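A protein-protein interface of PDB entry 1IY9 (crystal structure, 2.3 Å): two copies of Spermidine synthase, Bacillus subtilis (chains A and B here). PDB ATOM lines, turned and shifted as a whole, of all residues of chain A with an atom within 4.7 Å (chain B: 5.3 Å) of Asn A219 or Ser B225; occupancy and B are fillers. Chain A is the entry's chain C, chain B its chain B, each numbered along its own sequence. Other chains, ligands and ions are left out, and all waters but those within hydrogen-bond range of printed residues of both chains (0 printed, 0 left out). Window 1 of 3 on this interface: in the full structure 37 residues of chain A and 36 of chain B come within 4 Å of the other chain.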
ATOM      1  N   VAL A  60     -12.100  14.247   4.393  1.00  0.00           N
ATOM      2  CA  VAL A  60     -12.942  15.419   4.549  1.00  0.00           C
ATOM      3  C   VAL A  60     -12.805  16.397   3.389  1.00  0.00           C
ATOM      4  O   VAL A  60     -13.775  16.697   2.703  1.00  0.00           O
ATOM      5  CB  VAL A  60     -12.691  16.147   5.889  1.00  0.00           C
ATOM      6  CG1 VAL A  60     -13.679  17.300   6.040  1.00  0.00           C
ATOM      7  CG2 VAL A  60     -12.857  15.185   7.032  1.00  0.00           C
ATOM      8  N   ALA A 218     -16.444  22.685   6.711  1.00  0.00           N
ATOM      9  CA  ALA A 218     -16.062  21.296   6.995  1.00  0.00           C
ATOM     10  C   ALA A 218     -14.933  21.284   8.042  1.00  0.00           C
ATOM     11  O   ALA A 218     -14.137  22.248   8.137  1.00  0.00           O
ATOM     12  CB  ALA A 218     -15.606  20.567   5.721  1.00  0.00           C
ATOM     13  N   ASN A 219     -14.882  20.207   8.837  1.00  0.00           N
ATOM     14  CA  ASN A 219     -13.866  20.017   9.871  1.00  0.00           C
ATOM     15  C   ASN A 219     -12.661  19.225   9.371  1.00  0.00           C
ATOM     16  O   ASN A 219     -12.759  18.025   9.120  1.00  0.00           O
ATOM     17  CB  ASN A 219     -14.456  19.265  11.070  1.00  0.00           C
ATOM     18  CG  ASN A 219     -13.377  18.758  12.059  1.00  0.00           C
ATOM     19  OD1 ASN A 219     -12.473  19.504  12.473  1.00  0.00           O
ATOM     20  ND2 ASN A 219     -13.490  17.497  12.450  1.00  0.00           N
ATOM     21  N   ILE A 220     -11.513  19.881   9.264  1.00  0.00           N
ATOM     22  CA  ILE A 220     -10.282  19.206   8.851  1.00  0.00           C
ATOM     23  C   ILE A 220      -9.317  19.470  10.005  1.00  0.00           C
ATOM     24  O   ILE A 220      -8.728  20.541  10.091  1.00  0.00           O
ATOM     25  CB  ILE A 220      -9.736  19.780   7.529  1.00  0.00           C
ATOM     26  CG1 ILE A 220     -10.868  19.823   6.469  1.00  0.00           C
ATOM     27  CG2 ILE A 220      -8.570  18.904   7.022  1.00  0.00           C
ATOM     28  CD1 ILE A 220     -10.504  20.458   5.143  1.00  0.00           C
ATOM     29  N   PRO A 221      -9.148  18.489  10.906  1.00  0.00           N
ATOM     30  CA  PRO A 221      -8.279  18.554  12.089  1.00  0.00           C
ATOM     31  C   PRO A 221      -6.804  18.893  11.881  1.00  0.00           C
ATOM     32  O   PRO A 221      -6.136  19.396  12.792  1.00  0.00           O
ATOM     33  CB  PRO A 221      -8.480  17.185  12.747  1.00  0.00           C
ATOM     34  CG  PRO A 221      -8.812  16.299  11.609  1.00  0.00           C
ATOM     35  CD  PRO A 221      -9.748  17.151  10.772  1.00  0.00           C
ATOM     36  N   GLY A 226      -9.127  23.970  12.532  1.00  0.00           N
ATOM     37  CA  GLY A 226     -10.057  22.842  12.514  1.00  0.00           C
ATOM     38  C   GLY A 226     -11.340  23.069  11.725  1.00  0.00           C
ATOM     39  O   GLY A 226     -12.192  22.171  11.633  1.00  0.00           O
ATOM     40  N   TYR A 254     -17.477  11.165   5.354  1.00  0.00           N
ATOM     41  CA  TYR A 254     -17.843  12.449   5.935  1.00  0.00           C
ATOM     42  C   TYR A 254     -19.143  12.950   5.306  1.00  0.00           C
ATOM     43  O   TYR A 254     -20.171  13.088   5.986  1.00  0.00           O
ATOM     44  CB  TYR A 254     -16.735  13.474   5.687  1.00  0.00           C
ATOM     45  CG  TYR A 254     -16.923  14.784   6.417  1.00  0.00           C
ATOM     46  CD1 TYR A 254     -16.333  15.008   7.666  1.00  0.00           C
ATOM     47  CD2 TYR A 254     -17.696  15.792   5.871  1.00  0.00           C
ATOM     48  CE1 TYR A 254     -16.518  16.216   8.343  1.00  0.00           C
ATOM     49  CE2 TYR A 254     -17.890  16.992   6.529  1.00  0.00           C
ATOM     50  CZ  TYR A 254     -17.296  17.210   7.766  1.00  0.00           C
ATOM     51  OH  TYR A 254     -17.435  18.446   8.379  1.00  0.00           O
ATOM     52  N   GLN B   9      -2.242  16.701  22.742  1.00  0.00           N
ATOM     53  CA  GLN B   9      -3.622  16.251  22.755  1.00  0.00           C
ATOM     54  C   GLN B   9      -3.716  14.733  22.544  1.00  0.00           C
ATOM     55  O   GLN B   9      -4.762  14.135  22.723  1.00  0.00           O
ATOM     56  CB  GLN B   9      -4.374  16.981  21.655  1.00  0.00           C
ATOM     57  CG  GLN B   9      -4.330  18.486  21.801  1.00  0.00           C
ATOM     58  CD  GLN B   9      -4.818  19.207  20.559  1.00  0.00           C
ATOM     59  OE1 GLN B   9      -4.558  18.780  19.418  1.00  0.00           O
ATOM     60  NE2 GLN B   9      -5.527  20.312  20.769  1.00  0.00           N
ATOM     61  N   PHE B  13       0.416  13.961  18.808  1.00  0.00           N
ATOM     62  CA  PHE B  13      -0.098  15.138  18.133  1.00  0.00           C
ATOM     63  C   PHE B  13      -0.546  16.174  19.142  1.00  0.00           C
ATOM     64  O   PHE B  13      -1.033  15.829  20.210  1.00  0.00           O
ATOM     65  CB  PHE B  13      -1.294  14.721  17.259  1.00  0.00           C
ATOM     66  CG  PHE B  13      -2.001  15.865  16.574  1.00  0.00           C
ATOM     67  CD1 PHE B  13      -1.435  16.491  15.473  1.00  0.00           C
ATOM     68  CD2 PHE B  13      -3.262  16.288  17.006  1.00  0.00           C
ATOM     69  CE1 PHE B  13      -2.105  17.517  14.800  1.00  0.00           C
ATOM     70  CE2 PHE B  13      -3.946  17.321  16.333  1.00  0.00           C
ATOM     71  CZ  PHE B  13      -3.362  17.934  15.226  1.00  0.00           C
ATOM     72  N   ASN B 191     -14.030  14.585  21.243  1.00  0.00           N
ATOM     73  CA  ASN B 191     -13.977  14.621  19.804  1.00  0.00           C
ATOM     74  C   ASN B 191     -14.063  13.219  19.242  1.00  0.00           C
ATOM     75  O   ASN B 191     -13.728  12.254  19.922  1.00  0.00           O
ATOM     76  CB  ASN B 191     -12.674  15.298  19.334  1.00  0.00           C
ATOM     77  CG  ASN B 191     -11.445  14.443  19.587  1.00  0.00           C
ATOM     78  OD1 ASN B 191     -10.958  13.756  18.698  1.00  0.00           O
ATOM     79  ND2 ASN B 191     -10.954  14.464  20.806  1.00  0.00           N
ATOM     80  N   PRO B 192     -14.500  13.090  17.981  1.00  0.00           N
ATOM     81  CA  PRO B 192     -14.635  11.808  17.301  1.00  0.00           C
ATOM     82  C   PRO B 192     -13.373  11.277  16.633  1.00  0.00           C
ATOM     83  O   PRO B 192     -13.406  10.177  16.100  1.00  0.00           O
ATOM     84  CB  PRO B 192     -15.679  12.108  16.243  1.00  0.00           C
ATOM     85  CG  PRO B 192     -15.319  13.461  15.844  1.00  0.00           C
ATOM     86  CD  PRO B 192     -15.094  14.157  17.159  1.00  0.00           C
ATOM     87  N   TRP B 193     -12.280  12.031  16.637  1.00  0.00           N
ATOM     88  CA  TRP B 193     -11.060  11.576  15.989  1.00  0.00           C
ATOM     89  C   TRP B 193     -10.092  10.773  16.868  1.00  0.00           C
ATOM     90  O   TRP B 193      -9.445   9.828  16.396  1.00  0.00           O
ATOM     91  CB  TRP B 193     -10.292  12.768  15.407  1.00  0.00           C
ATOM     92  CG  TRP B 193     -10.999  13.492  14.333  1.00  0.00           C
ATOM     93  CD1 TRP B 193     -11.865  14.534  14.491  1.00  0.00           C
ATOM     94  CD2 TRP B 193     -10.917  13.244  12.916  1.00  0.00           C
ATOM     95  NE1 TRP B 193     -12.335  14.945  13.272  1.00  0.00           N
ATOM     96  CE2 TRP B 193     -11.775  14.175  12.280  1.00  0.00           C
ATOM     97  CE3 TRP B 193     -10.202  12.329  12.124  1.00  0.00           C
ATOM     98  CZ2 TRP B 193     -11.947  14.221  10.882  1.00  0.00           C
ATOM     99  CZ3 TRP B 193     -10.368  12.366  10.734  1.00  0.00           C
ATOM    100  CH2 TRP B 193     -11.239  13.313  10.132  1.00  0.00           C
ATOM    101  N   PHE B 194      -9.944  11.176  18.124  1.00  0.00           N
ATOM    102  CA  PHE B 194      -8.985  10.509  19.000  1.00  0.00           C
ATOM    103  C   PHE B 194      -9.602   9.715  20.153  1.00  0.00           C
ATOM    104  O   PHE B 194      -9.000   8.775  20.688  1.00  0.00           O
ATOM    105  CB  PHE B 194      -7.957  11.531  19.516  1.00  0.00           C
ATOM    106  CG  PHE B 194      -7.431  12.475  18.444  1.00  0.00           C
ATOM    107  CD1 PHE B 194      -7.489  13.856  18.630  1.00  0.00           C
ATOM    108  CD2 PHE B 194      -6.922  11.992  17.242  1.00  0.00           C
ATOM    109  CE1 PHE B 194      -7.058  14.747  17.634  1.00  0.00           C
ATOM    110  CE2 PHE B 194      -6.489  12.868  16.241  1.00  0.00           C
ATOM    111  CZ  PHE B 194      -6.562  14.257  16.441  1.00  0.00           C
ATOM    112  N   TYR B 223      -9.380  23.015  20.977  1.00  0.00           N
ATOM    113  CA  TYR B 223      -9.644  21.696  21.541  1.00  0.00           C
ATOM    114  C   TYR B 223      -9.219  20.647  20.532  1.00  0.00           C
ATOM    115  O   TYR B 223      -9.248  20.886  19.316  1.00  0.00           O
ATOM    116  CB  TYR B 223     -11.129  21.527  21.851  1.00  0.00           C
ATOM    117  CG  TYR B 223     -11.602  22.158  23.131  1.00  0.00           C
ATOM    118  CD1 TYR B 223     -10.786  23.015  23.865  1.00  0.00           C
ATOM    119  CD2 TYR B 223     -12.882  21.878  23.629  1.00  0.00           C
ATOM    120  CE1 TYR B 223     -11.247  23.579  25.073  1.00  0.00           C
ATOM    121  CE2 TYR B 223     -13.349  22.418  24.822  1.00  0.00           C
ATOM    122  CZ  TYR B 223     -12.536  23.260  25.537  1.00  0.00           C
ATOM    123  OH  TYR B 223     -13.022  23.749  26.728  1.00  0.00           O
ATOM    124  N   PRO B 224      -8.879  19.439  21.019  1.00  0.00           N
ATOM    125  CA  PRO B 224      -8.448  18.346  20.137  1.00  0.00           C
ATOM    126  C   PRO B 224      -9.292  18.124  18.862  1.00  0.00           C
ATOM    127  O   PRO B 224     -10.503  17.919  18.924  1.00  0.00           O
ATOM    128  CB  PRO B 224      -8.449  17.138  21.071  1.00  0.00           C
ATOM    129  CG  PRO B 224      -8.031  17.744  22.370  1.00  0.00           C
ATOM    130  CD  PRO B 224      -8.860  19.019  22.435  1.00  0.00           C
ATOM    131  N   SER B 225      -8.622  18.195  17.717  1.00  0.00           N
ATOM    132  CA  SER B 225      -9.196  17.998  16.394  1.00  0.00           C
ATOM    133  C   SER B 225     -10.024  19.137  15.812  1.00  0.00           C
ATOM    134  O   SER B 225     -10.362  19.111  14.621  1.00  0.00           O
ATOM    135  CB  SER B 225      -9.982  16.695  16.315  1.00  0.00           C
ATOM    136  OG  SER B 225     -11.302  16.844  16.805  1.00  0.00           O
ATOM    137  N   GLY B 226     -10.366  20.124  16.631  1.00  0.00           N
ATOM    138  CA  GLY B 226     -11.139  21.240  16.125  1.00  0.00           C
ATOM    139  C   GLY B 226     -12.625  20.969  16.050  1.00  0.00           C
ATOM    140  O   GLY B 226     -13.417  21.846  15.691  1.00  0.00           O
ATOM    141  N   LEU B 227     -13.024  19.755  16.393  1.00  0.00           N
ATOM    142  CA  LEU B 227     -14.441  19.390  16.370  1.00  0.00           C
ATOM    143  C   LEU B 227     -14.775  18.801  17.725  1.00  0.00           C
ATOM    144  O   LEU B 227     -14.182  17.799  18.123  1.00  0.00           O
ATOM    145  CB  LEU B 227     -14.725  18.351  15.284  1.00  0.00           C
ATOM    146  CG  LEU B 227     -16.189  17.939  15.133  1.00  0.00           C
ATOM    147  CD1 LEU B 227     -16.989  19.159  14.713  1.00  0.00           C
ATOM    148  CD2 LEU B 227     -16.342  16.844  14.089  1.00  0.00           C
ATOM    149  N   PHE B 269     -18.844   9.599   9.356  1.00  0.00           N
ATOM    150  CA  PHE B 269     -18.057   8.812  10.299  1.00  0.00           C
ATOM    151  C   PHE B 269     -18.421   9.040  11.745  1.00  0.00           C
ATOM    152  O   PHE B 269     -18.101   8.210  12.588  1.00  0.00           O
ATOM    153  CB  PHE B 269     -16.545   8.985  10.082  1.00  0.00           C
ATOM    154  CG  PHE B 269     -15.967  10.220  10.715  1.00  0.00           C
ATOM    155  CD1 PHE B 269     -15.280  10.135  11.928  1.00  0.00           C
ATOM    156  CD2 PHE B 269     -16.117  11.473  10.116  1.00  0.00           C
ATOM    157  CE1 PHE B 269     -14.750  11.276  12.541  1.00  0.00           C
ATOM    158  CE2 PHE B 269     -15.594  12.622  10.716  1.00  0.00           C
ATOM    159  CZ  PHE B 269     -14.910  12.522  11.935  1.00  0.00           C
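Among the printed residues, pairs that only touch across the chains: Val A60 with Trp B193 (3.97 Å), Asn A219 with Gly B226 (3.9 Å), Asn A219 with Leu B227 (3.2 Å), Pro A221 with Phe B13 (3.97 Å), Pro A221 with Trp B193 (3.7 Å), Pro A221 with Ser B225 (3.3 Å) and Tyr A254 with Phe B269 (3.9 Å).
Printed residues of chain B within 4 Å of Val A60: Trp B193 (3.97 Å).
Asn A219 touches just these residues of chain B: Trp B193, Ser B225, Gly B226 and Leu B227.
Of the printed residues of chain B, Pro A221 touches Phe B13, Trp B193 and Ser B225.
Of the printed residues of chain A, Ser B225 touches Asn A219 (3.0 Å) and Pro A221 (3.3 Å).
The nearest residue of chain B that does not touch Asn A219 is Phe B269 (5.2 Å).
The nearest printed residue of chain A that does not touch Gly B226 is Gly A226 (4.1 Å).
Of the 7 printed residues of chain A, 4 touch a printed residue of chain B.
Printed residues of chain A that touch a printed residue of chain B: Val A60, Asn A219, Pro A221 and Tyr A254.
Hydrophobic or aromatic side chains of chain B within 4 Å of the printed part of chain A: Phe B13, Trp B193, Leu B227 and Phe B269.
Among the printed residues, no Asp or Glu carboxylate lies within 4 Å of a Lys or Arg side-chain nitrogen of the other chain.
The side-chain amide oxygen of Asn A219 lies close to the backbone carbonyl oxygen of Gly A226 (2.8 Å).
O of Leu B227 is in hydrogen-bond range of OG of Ser B225.
The side-chain amide oxygen (OD1) of Asn B191 lies within hydrogen-bond range of the backbone NH (N) of Trp B193.
The side-chain hydroxyl (OH) of Tyr A254 is in hydrogen-bond range of the backbone NH (N) of Asn A219, 3.1 Å away.
1 position is printed for both chains.
Of the 9 pairs that touch across the chains among the printed residues, none has its exchanged pair printed and touching as well.
The backbone carbonyl oxygen of Ser B225 lies close to the side-chain amide oxygen of Asn A219, at 3.0 Å.
NE1 of Trp B193 lies close to ND2 of Asn A219.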
